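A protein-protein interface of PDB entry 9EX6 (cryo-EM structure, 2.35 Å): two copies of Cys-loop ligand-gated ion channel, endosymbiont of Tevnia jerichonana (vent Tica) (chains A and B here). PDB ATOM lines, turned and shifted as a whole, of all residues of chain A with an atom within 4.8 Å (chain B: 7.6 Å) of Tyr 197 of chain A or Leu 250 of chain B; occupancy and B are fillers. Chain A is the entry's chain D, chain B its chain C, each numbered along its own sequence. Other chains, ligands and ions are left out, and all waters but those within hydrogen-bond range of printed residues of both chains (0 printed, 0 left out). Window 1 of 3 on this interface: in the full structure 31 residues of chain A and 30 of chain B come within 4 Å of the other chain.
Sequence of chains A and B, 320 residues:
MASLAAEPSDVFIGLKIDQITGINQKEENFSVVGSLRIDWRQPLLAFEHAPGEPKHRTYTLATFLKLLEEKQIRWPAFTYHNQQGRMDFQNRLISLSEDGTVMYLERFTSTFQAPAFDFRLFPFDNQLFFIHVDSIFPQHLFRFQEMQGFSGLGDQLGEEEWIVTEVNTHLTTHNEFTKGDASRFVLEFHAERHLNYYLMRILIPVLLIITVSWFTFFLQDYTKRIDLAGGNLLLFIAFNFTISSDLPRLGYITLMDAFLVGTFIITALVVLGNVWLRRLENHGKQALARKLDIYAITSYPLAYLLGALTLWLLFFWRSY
OH of Tyr 197 of chain A lies within hydrogen-bond range of O of Leu 250 of chain B (3.5 Å).
The backbone NH (N) of Thr 254 of chain B sits at hydrogen-bond distance from the side-chain carboxylate (OD2) of Asp 257 of chain B. The side-chain carboxylate (OD1) of Asp 246 of chain A is in hydrogen-bond range of the side-chain hydroxyl (OH) of Tyr 197 of chain A. The backbone NH of Phe 119 of chain B sits at hydrogen-bond distance from the side-chain hydroxyl of Tyr 252 of chain B.
CD2 of His 194 of chain A touches O of Gly 251 of chain B, 3.7 Å away. OD1 of Asn 196 of chain A touches CD1 of Ile 253 of chain B (3.6 Å). CG of Tyr 197 of chain A touches O of Gly 251 of chain B (3.8 Å). CD1 of Tyr 197 of chain A touches C of Tyr 252 of chain B (3.6 Å). Met 200 of chain A touches Ile 253 of chain B. Asp 257 of chain B touches Met 200 of chain A (CB to CE, 3.6 Å). O of Met 200 of chain A touches CG2 of Val 261 of chain B, 3.9 Å away.
Printed residues of chain B within 4 Å of Tyr 197 of chain A: Leu 250, Gly 251 and Tyr 252. Leu 250 of chain B touches just one residue of chain A: Tyr 197 (3.5 Å). Of the printed residues of chain A, Val 261 of chain B touches Met 200. Of the printed residues of chain A, Ile 253 of chain B touches Asn 196 and Met 200. The nearest printed residue of chain B that does not touch Tyr 197 of chain A is Ile 253 of chain B (4.01 Å). The nearest printed residue of chain A that does not touch Val 261 of chain B is Arg 201 of chain A (5.1 Å).
Hydrophobic or aromatic side chains of chain B within 4 Å of the printed part of chain A: Ile 253 and Val 261. Of the 9 printed residues of chain A, 4 touch a printed residue of chain B. Hydrophobic or aromatic side chains of chain A that line the printed part of chain B: His 194, Tyr 197 and Met 200. Among the printed residues, 8 pairs touch across the chains.
No position is printed for both chains. Of the 8 pairs that touch across the chains among the printed residues, none has its exchanged pair printed and touching as well.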
ATOM      1  N   HIS A 194     -25.704  20.967  20.336  1.00  0.00           N
ATOM      2  CA  HIS A 194     -25.048  21.110  19.024  1.00  0.00           C
ATOM      3  C   HIS A 194     -26.121  21.134  17.936  1.00  0.00           C
ATOM      4  O   HIS A 194     -26.654  20.089  17.560  1.00  0.00           O
ATOM      5  CB  HIS A 194     -24.094  19.950  18.720  1.00  0.00           C
ATOM      6  CG  HIS A 194     -22.958  19.771  19.685  1.00  0.00           C
ATOM      7  ND1 HIS A 194     -21.728  20.360  19.488  1.00  0.00           N
ATOM      8  CD2 HIS A 194     -22.832  18.999  20.792  1.00  0.00           C
ATOM      9  CE1 HIS A 194     -20.912  20.008  20.467  1.00  0.00           C
ATOM     10  NE2 HIS A 194     -21.555  19.180  21.269  1.00  0.00           N
ATOM     11  N   LEU A 195     -26.410  22.313  17.375  1.00  0.00           N
ATOM     12  CA  LEU A 195     -27.432  22.395  16.329  1.00  0.00           C
ATOM     13  C   LEU A 195     -26.955  21.769  15.022  1.00  0.00           C
ATOM     14  O   LEU A 195     -27.769  21.287  14.224  1.00  0.00           O
ATOM     15  CB  LEU A 195     -27.824  23.852  16.103  1.00  0.00           C
ATOM     16  CG  LEU A 195     -28.709  24.571  17.127  1.00  0.00           C
ATOM     17  CD1 LEU A 195     -28.617  26.100  17.014  1.00  0.00           C
ATOM     18  CD2 LEU A 195     -30.130  24.033  17.194  1.00  0.00           C
ATOM     19  N   ASN A 196     -25.643  21.818  14.792  1.00  0.00           N
ATOM     20  CA  ASN A 196     -24.966  21.144  13.686  1.00  0.00           C
ATOM     21  C   ASN A 196     -25.470  19.713  13.481  1.00  0.00           C
ATOM     22  O   ASN A 196     -25.699  19.272  12.346  1.00  0.00           O
ATOM     23  CB  ASN A 196     -23.471  21.188  14.021  1.00  0.00           C
ATOM     24  CG  ASN A 196     -22.572  20.732  12.911  1.00  0.00           C
ATOM     25  OD1 ASN A 196     -22.978  20.586  11.758  1.00  0.00           O
ATOM     26  ND2 ASN A 196     -21.320  20.458  13.273  1.00  0.00           N
ATOM     27  N   TYR A 197     -25.673  18.986  14.584  1.00  0.00           N
ATOM     28  CA  TYR A 197     -26.067  17.582  14.521  1.00  0.00           C
ATOM     29  C   TYR A 197     -27.487  17.427  13.991  1.00  0.00           C
ATOM     30  O   TYR A 197     -27.766  16.512  13.209  1.00  0.00           O
ATOM     31  CB  TYR A 197     -25.934  16.965  15.910  1.00  0.00           C
ATOM     32  CG  TYR A 197     -26.504  15.576  16.100  1.00  0.00           C
ATOM     33  CD1 TYR A 197     -25.770  14.451  15.765  1.00  0.00           C
ATOM     34  CD2 TYR A 197     -27.758  15.392  16.657  1.00  0.00           C
ATOM     35  CE1 TYR A 197     -26.283  13.181  15.948  1.00  0.00           C
ATOM     36  CE2 TYR A 197     -28.288  14.129  16.815  1.00  0.00           C
ATOM     37  CZ  TYR A 197     -27.526  13.022  16.522  1.00  0.00           C
ATOM     38  OH  TYR A 197     -28.047  11.759  16.700  1.00  0.00           O
ATOM     39  N   TYR A 198     -28.377  18.353  14.348  1.00  0.00           N
ATOM     40  CA  TYR A 198     -29.766  18.231  13.931  1.00  0.00           C
ATOM     41  C   TYR A 198     -29.958  18.705  12.501  1.00  0.00           C
ATOM     42  O   TYR A 198     -30.827  18.184  11.795  1.00  0.00           O
ATOM     43  CB  TYR A 198     -30.667  18.986  14.909  1.00  0.00           C
ATOM     44  CG  TYR A 198     -30.687  18.334  16.279  1.00  0.00           C
ATOM     45  CD1 TYR A 198     -31.557  17.291  16.559  1.00  0.00           C
ATOM     46  CD2 TYR A 198     -29.812  18.738  17.278  1.00  0.00           C
ATOM     47  CE1 TYR A 198     -31.573  16.687  17.804  1.00  0.00           C
ATOM     48  CE2 TYR A 198     -29.825  18.139  18.523  1.00  0.00           C
ATOM     49  CZ  TYR A 198     -30.686  17.092  18.767  1.00  0.00           C
ATOM     50  OH  TYR A 198     -30.716  16.495  20.006  1.00  0.00           O
ATOM     51  N   LEU A 199     -29.137  19.659  12.057  1.00  0.00           N
ATOM     52  CA  LEU A 199     -29.129  20.042  10.650  1.00  0.00           C
ATOM     53  C   LEU A 199     -28.826  18.835   9.771  1.00  0.00           C
ATOM     54  O   LEU A 199     -29.566  18.541   8.823  1.00  0.00           O
ATOM     55  CB  LEU A 199     -28.111  21.162  10.422  1.00  0.00           C
ATOM     56  CG  LEU A 199     -27.650  21.482   8.997  1.00  0.00           C
ATOM     57  CD1 LEU A 199     -28.794  21.986   8.136  1.00  0.00           C
ATOM     58  CD2 LEU A 199     -26.508  22.484   9.019  1.00  0.00           C
ATOM     59  N   MET A 200     -27.787  18.071  10.139  1.00  0.00           N
ATOM     60  CA  MET A 200     -27.344  16.942   9.324  1.00  0.00           C
ATOM     61  C   MET A 200     -28.315  15.772   9.408  1.00  0.00           C
ATOM     62  O   MET A 200     -28.579  15.099   8.405  1.00  0.00           O
ATOM     63  CB  MET A 200     -25.950  16.489   9.762  1.00  0.00           C
ATOM     64  CG  MET A 200     -25.149  15.790   8.672  1.00  0.00           C
ATOM     65  SD  MET A 200     -23.556  15.138   9.226  1.00  0.00           S
ATOM     66  CE  MET A 200     -24.069  13.733  10.203  1.00  0.00           C
ATOM     67  N   ARG A 201     -28.823  15.490  10.599  1.00  0.00           N
ATOM     68  CA  ARG A 201     -29.665  14.304  10.769  1.00  0.00           C
ATOM     69  C   ARG A 201     -31.118  14.442  10.369  1.00  0.00           C
ATOM     70  O   ARG A 201     -31.746  13.442  10.016  1.00  0.00           O
ATOM     71  CB  ARG A 201     -29.626  13.872  12.241  1.00  0.00           C
ATOM     72  CG  ARG A 201     -28.387  13.084  12.626  1.00  0.00           C
ATOM     73  CD  ARG A 201     -28.463  11.658  12.109  1.00  0.00           C
ATOM     74  NE  ARG A 201     -29.400  10.838  12.876  1.00  0.00           N
ATOM     75  CZ  ARG A 201     -30.488  10.263  12.370  1.00  0.00           C
ATOM     76  NH1 ARG A 201     -30.794  10.414  11.087  1.00  0.00           N
ATOM     77  NH2 ARG A 201     -31.274   9.533  13.149  1.00  0.00           N
ATOM     78  N   ASP A 246     -34.045  10.076  18.352  1.00  0.00           N
ATOM     79  CA  ASP A 246     -33.498  11.400  18.597  1.00  0.00           C
ATOM     80  C   ASP A 246     -34.534  12.361  19.161  1.00  0.00           C
ATOM     81  O   ASP A 246     -34.164  13.468  19.557  1.00  0.00           O
ATOM     82  CB  ASP A 246     -32.933  12.009  17.299  1.00  0.00           C
ATOM     83  CG  ASP A 246     -31.588  11.442  16.900  1.00  0.00           C
ATOM     84  OD1 ASP A 246     -30.637  11.522  17.703  1.00  0.00           O
ATOM     85  OD2 ASP A 246     -31.467  10.967  15.752  1.00  0.00           O
ATOM     86  N   GLN B  25     -21.021   4.206  26.999  1.00  0.00           N
ATOM     87  CA  GLN B  25     -20.555   5.226  26.064  1.00  0.00           C
ATOM     88  C   GLN B  25     -21.333   6.536  26.191  1.00  0.00           C
ATOM     89  O   GLN B  25     -20.769   7.605  25.924  1.00  0.00           O
ATOM     90  CB  GLN B  25     -20.620   4.677  24.634  1.00  0.00           C
ATOM     91  CG  GLN B  25     -19.685   3.484  24.382  1.00  0.00           C
ATOM     92  CD  GLN B  25     -19.845   2.859  23.004  1.00  0.00           C
ATOM     93  OE1 GLN B  25     -18.884   2.769  22.233  1.00  0.00           O
ATOM     94  NE2 GLN B  25     -21.058   2.406  22.695  1.00  0.00           N
ATOM     95  N   LYS B  26     -22.591   6.481  26.636  1.00  0.00           N
ATOM     96  CA  LYS B  26     -23.410   7.684  26.770  1.00  0.00           C
ATOM     97  C   LYS B  26     -23.130   8.418  28.082  1.00  0.00           C
ATOM     98  O   LYS B  26     -23.056   9.652  28.094  1.00  0.00           O
ATOM     99  CB  LYS B  26     -24.892   7.307  26.648  1.00  0.00           C
ATOM    100  CG  LYS B  26     -25.878   8.468  26.583  1.00  0.00           C
ATOM    101  CD  LYS B  26     -27.303   7.999  26.208  1.00  0.00           C
ATOM    102  CE  LYS B  26     -28.219   9.194  25.978  1.00  0.00           C
ATOM    103  NZ  LYS B  26     -28.544   9.878  27.261  1.00  0.00           N
ATOM    104  N   GLU B  27     -22.951   7.681  29.183  1.00  0.00           N
ATOM    105  CA  GLU B  27     -22.644   8.279  30.480  1.00  0.00           C
ATOM    106  C   GLU B  27     -21.161   8.572  30.672  1.00  0.00           C
ATOM    107  O   GLU B  27     -20.811   9.344  31.572  1.00  0.00           O
ATOM    108  CB  GLU B  27     -23.099   7.359  31.617  1.00  0.00           C
ATOM    109  CG  GLU B  27     -24.592   7.227  31.791  1.00  0.00           C
ATOM    110  CD  GLU B  27     -24.974   6.420  33.024  1.00  0.00           C
ATOM    111  OE1 GLU B  27     -24.105   5.745  33.615  1.00  0.00           O
ATOM    112  OE2 GLU B  27     -26.174   6.394  33.363  1.00  0.00           O
ATOM    113  N   GLU B  28     -20.294   7.949  29.871  1.00  0.00           N
ATOM    114  CA  GLU B  28     -18.838   8.078  29.968  1.00  0.00           C
ATOM    115  C   GLU B  28     -18.316   7.589  31.329  1.00  0.00           C
ATOM    116  O   GLU B  28     -17.815   8.363  32.146  1.00  0.00           O
ATOM    117  CB  GLU B  28     -18.401   9.525  29.668  1.00  0.00           C
ATOM    118  CG  GLU B  28     -18.797  10.009  28.255  1.00  0.00           C
ATOM    119  CD  GLU B  28     -18.113  11.303  27.819  1.00  0.00           C
ATOM    120  OE1 GLU B  28     -17.347  11.892  28.609  1.00  0.00           O
ATOM    121  OE2 GLU B  28     -18.365  11.746  26.678  1.00  0.00           O
ATOM    122  N   ASP B 118     -14.067   9.980  23.580  1.00  0.00           N
ATOM    123  CA  ASP B 118     -14.347  10.818  22.404  1.00  0.00           C
ATOM    124  C   ASP B 118     -14.571   9.904  21.207  1.00  0.00           C
ATOM    125  O   ASP B 118     -13.647   9.206  20.784  1.00  0.00           O
ATOM    126  CB  ASP B 118     -13.194  11.819  22.156  1.00  0.00           C
ATOM    127  CG  ASP B 118     -13.259  12.510  20.792  1.00  0.00           C
ATOM    128  OD1 ASP B 118     -14.325  12.515  20.149  1.00  0.00           O
ATOM    129  OD2 ASP B 118     -12.252  13.141  20.411  1.00  0.00           O
ATOM    130  N   PHE B 119     -15.785   9.921  20.645  1.00  0.00           N
ATOM    131  CA  PHE B 119     -16.218   8.912  19.679  1.00  0.00           C
ATOM    132  C   PHE B 119     -16.372   9.455  18.257  1.00  0.00           C
ATOM    133  O   PHE B 119     -17.057   8.835  17.438  1.00  0.00           O
ATOM    134  CB  PHE B 119     -17.526   8.268  20.146  1.00  0.00           C
ATOM    135  CG  PHE B 119     -17.406   7.536  21.455  1.00  0.00           C
ATOM    136  CD1 PHE B 119     -16.787   6.301  21.521  1.00  0.00           C
ATOM    137  CD2 PHE B 119     -17.902   8.096  22.621  1.00  0.00           C
ATOM    138  CE1 PHE B 119     -16.668   5.629  22.726  1.00  0.00           C
ATOM    139  CE2 PHE B 119     -17.773   7.437  23.836  1.00  0.00           C
ATOM    140  CZ  PHE B 119     -17.166   6.195  23.884  1.00  0.00           C
ATOM    141  N   ARG B 120     -15.714  10.569  17.931  1.00  0.00           N
ATOM    142  CA  ARG B 120     -15.923  11.191  16.624  1.00  0.00           C
ATOM    143  C   ARG B 120     -15.399  10.341  15.466  1.00  0.00           C
ATOM    144  O   ARG B 120     -15.895  10.464  14.339  1.00  0.00           O
ATOM    145  CB  ARG B 120     -15.274  12.575  16.603  1.00  0.00           C
ATOM    146  CG  ARG B 120     -16.039  13.672  17.331  1.00  0.00           C
ATOM    147  CD  ARG B 120     -15.284  14.993  17.405  1.00  0.00           C
ATOM    148  NE  ARG B 120     -14.138  14.940  18.304  1.00  0.00           N
ATOM    149  CZ  ARG B 120     -13.382  15.986  18.612  1.00  0.00           C
ATOM    150  NH1 ARG B 120     -13.622  17.185  18.111  1.00  0.00           N
ATOM    151  NH2 ARG B 120     -12.371  15.825  19.460  1.00  0.00           N
ATOM    152  N   PHE B 122     -15.546   7.034  15.264  1.00  0.00           N
ATOM    153  CA  PHE B 122     -16.231   5.749  15.262  1.00  0.00           C
ATOM    154  C   PHE B 122     -16.501   5.281  13.829  1.00  0.00           C
ATOM    155  O   PHE B 122     -16.994   6.070  13.003  1.00  0.00           O
ATOM    156  CB  PHE B 122     -17.544   5.880  16.045  1.00  0.00           C
ATOM    157  CG  PHE B 122     -18.405   4.646  16.010  1.00  0.00           C
ATOM    158  CD1 PHE B 122     -18.281   3.630  16.900  1.00  0.00           C
ATOM    159  CD2 PHE B 122     -19.444   4.587  15.054  1.00  0.00           C
ATOM    160  CE1 PHE B 122     -19.121   2.503  16.856  1.00  0.00           C
ATOM    161  CE2 PHE B 122     -20.238   3.505  14.981  1.00  0.00           C
ATOM    162  CZ  PHE B 122     -20.122   2.469  15.875  1.00  0.00           C
ATOM    163  N   ARG B 193     -11.908  -1.624  19.015  1.00  0.00           N
ATOM    164  CA  ARG B 193     -12.982  -2.525  18.577  1.00  0.00           C
ATOM    165  C   ARG B 193     -12.513  -3.563  17.544  1.00  0.00           C
ATOM    166  O   ARG B 193     -11.422  -3.470  16.983  1.00  0.00           O
ATOM    167  CB  ARG B 193     -14.142  -1.719  17.968  1.00  0.00           C
ATOM    168  CG  ARG B 193     -14.701  -0.602  18.833  1.00  0.00           C
ATOM    169  CD  ARG B 193     -15.713   0.259  18.069  1.00  0.00           C
ATOM    170  NE  ARG B 193     -15.890   1.559  18.708  1.00  0.00           N
ATOM    171  CZ  ARG B 193     -16.798   1.830  19.637  1.00  0.00           C
ATOM    172  NH1 ARG B 193     -17.692   0.932  20.016  1.00  0.00           N
ATOM    173  NH2 ARG B 193     -16.798   3.028  20.210  1.00  0.00           N
ATOM    174  N   LEU B 247     -25.526   1.505  16.517  1.00  0.00           N
ATOM    175  CA  LEU B 247     -25.066   2.892  16.491  1.00  0.00           C
ATOM    176  C   LEU B 247     -25.264   3.538  17.852  1.00  0.00           C
ATOM    177  O   LEU B 247     -26.377   3.482  18.387  1.00  0.00           O
ATOM    178  CB  LEU B 247     -25.806   3.684  15.413  1.00  0.00           C
ATOM    179  CG  LEU B 247     -25.709   3.103  13.997  1.00  0.00           C
ATOM    180  CD1 LEU B 247     -26.591   3.862  13.017  1.00  0.00           C
ATOM    181  CD2 LEU B 247     -24.261   3.048  13.507  1.00  0.00           C
ATOM    182  N   PRO B 248     -24.252   4.154  18.458  1.00  0.00           N
ATOM    183  CA  PRO B 248     -24.438   4.726  19.794  1.00  0.00           C
ATOM    184  C   PRO B 248     -25.207   6.042  19.777  1.00  0.00           C
ATOM    185  O   PRO B 248     -25.157   6.811  18.816  1.00  0.00           O
ATOM    186  CB  PRO B 248     -22.999   4.925  20.286  1.00  0.00           C
ATOM    187  CG  PRO B 248     -22.228   5.223  19.047  1.00  0.00           C
ATOM    188  CD  PRO B 248     -22.858   4.296  17.993  1.00  0.00           C
ATOM    189  N   ARG B 249     -25.931   6.289  20.875  1.00  0.00           N
ATOM    190  CA  ARG B 249     -26.853   7.424  20.982  1.00  0.00           C
ATOM    191  C   ARG B 249     -26.117   8.608  21.603  1.00  0.00           C
ATOM    192  O   ARG B 249     -26.092   8.793  22.820  1.00  0.00           O
ATOM    193  CB  ARG B 249     -28.086   7.048  21.794  1.00  0.00           C
ATOM    194  CG  ARG B 249     -29.107   6.150  21.079  1.00  0.00           C
ATOM    195  CD  ARG B 249     -30.301   5.919  22.012  1.00  0.00           C
ATOM    196  NE  ARG B 249     -31.257   4.934  21.514  1.00  0.00           N
ATOM    197  CZ  ARG B 249     -32.524   4.867  21.900  1.00  0.00           C
ATOM    198  NH1 ARG B 249     -33.005   5.627  22.867  1.00  0.00           N
ATOM    199  NH2 ARG B 249     -33.329   3.987  21.305  1.00  0.00           N
ATOM    200  N   LEU B 250     -25.553   9.441  20.737  1.00  0.00           N
ATOM    201  CA  LEU B 250     -24.663  10.541  21.069  1.00  0.00           C
ATOM    202  C   LEU B 250     -25.241  11.823  20.483  1.00  0.00           C
ATOM    203  O   LEU B 250     -25.908  11.791  19.447  1.00  0.00           O
ATOM    204  CB  LEU B 250     -23.276  10.271  20.502  1.00  0.00           C
ATOM    205  CG  LEU B 250     -22.495   9.068  21.043  1.00  0.00           C
ATOM    206  CD1 LEU B 250     -21.117   9.028  20.416  1.00  0.00           C
ATOM    207  CD2 LEU B 250     -22.426   8.999  22.559  1.00  0.00           C
ATOM    208  N   GLY B 251     -25.009  12.953  21.142  1.00  0.00           N
ATOM    209  CA  GLY B 251     -25.613  14.164  20.622  1.00  0.00           C
ATOM    210  C   GLY B 251     -24.721  14.961  19.694  1.00  0.00           C
ATOM    211  O   GLY B 251     -24.927  16.164  19.514  1.00  0.00           O
ATOM    212  N   TYR B 252     -23.758  14.291  19.059  1.00  0.00           N
ATOM    213  CA  TYR B 252     -22.806  14.955  18.177  1.00  0.00           C
ATOM    214  C   TYR B 252     -22.410  14.044  17.018  1.00  0.00           C
ATOM    215  O   TYR B 252     -22.646  12.836  17.044  1.00  0.00           O
ATOM    216  CB  TYR B 252     -21.566  15.416  18.951  1.00  0.00           C
ATOM    217  CG  TYR B 252     -20.787  14.339  19.690  1.00  0.00           C
ATOM    218  CD1 TYR B 252     -19.720  13.697  19.079  1.00  0.00           C
ATOM    219  CD2 TYR B 252     -21.007  14.086  21.039  1.00  0.00           C
ATOM    220  CE1 TYR B 252     -18.975  12.744  19.744  1.00  0.00           C
ATOM    221  CE2 TYR B 252     -20.253  13.138  21.722  1.00  0.00           C
ATOM    222  CZ  TYR B 252     -19.240  12.468  21.065  1.00  0.00           C
ATOM    223  OH  TYR B 252     -18.487  11.517  21.720  1.00  0.00           O
ATOM    224  N   ILE B 253     -21.763  14.648  16.003  1.00  0.00           N
ATOM    225  CA  ILE B 253     -21.551  14.009  14.702  1.00  0.00           C
ATOM    226  C   ILE B 253     -20.359  13.054  14.742  1.00  0.00           C
ATOM    227  O   ILE B 253     -19.293  13.389  15.269  1.00  0.00           O
ATOM    228  CB  ILE B 253     -21.357  15.078  13.608  1.00  0.00           C
ATOM    229  CG1 ILE B 253     -22.669  15.821  13.333  1.00  0.00           C
ATOM    230  CG2 ILE B 253     -20.875  14.430  12.330  1.00  0.00           C
ATOM    231  CD1 ILE B 253     -22.501  17.029  12.422  1.00  0.00           C
ATOM    232  N   THR B 254     -20.535  11.859  14.163  1.00  0.00           N
ATOM    233  CA  THR B 254     -19.481  10.863  13.987  1.00  0.00           C
ATOM    234  C   THR B 254     -19.159  10.663  12.509  1.00  0.00           C
ATOM    235  O   THR B 254     -19.919  11.051  11.620  1.00  0.00           O
ATOM    236  CB  THR B 254     -19.874   9.506  14.585  1.00  0.00           C
ATOM    237  OG1 THR B 254     -21.092   9.077  13.977  1.00  0.00           O
ATOM    238  CG2 THR B 254     -20.116   9.635  16.077  1.00  0.00           C
ATOM    239  N   ASP B 257     -21.904   8.705  10.896  1.00  0.00           N
ATOM    240  CA  ASP B 257     -23.075   9.511  10.568  1.00  0.00           C
ATOM    241  C   ASP B 257     -22.910  10.208   9.223  1.00  0.00           C
ATOM    242  O   ASP B 257     -23.830  10.211   8.394  1.00  0.00           O
ATOM    243  CB  ASP B 257     -23.347  10.547  11.660  1.00  0.00           C
ATOM    244  CG  ASP B 257     -23.681   9.926  13.002  1.00  0.00           C
ATOM    245  OD1 ASP B 257     -24.535   9.020  13.075  1.00  0.00           O
ATOM    246  OD2 ASP B 257     -23.067  10.365  13.999  1.00  0.00           O
ATOM    247  N   VAL B 261     -25.332   9.786   5.704  1.00  0.00           N
ATOM    248  CA  VAL B 261     -26.080  10.914   5.148  1.00  0.00           C
ATOM    249  C   VAL B 261     -25.641  11.193   3.714  1.00  0.00           C
ATOM    250  O   VAL B 261     -26.452  11.597   2.865  1.00  0.00           O
ATOM    251  CB  VAL B 261     -25.928  12.168   6.028  1.00  0.00           C
ATOM    252  CG1 VAL B 261     -26.679  13.323   5.384  1.00  0.00           C
ATOM    253  CG2 VAL B 261     -26.552  11.921   7.381  1.00  0.00           C
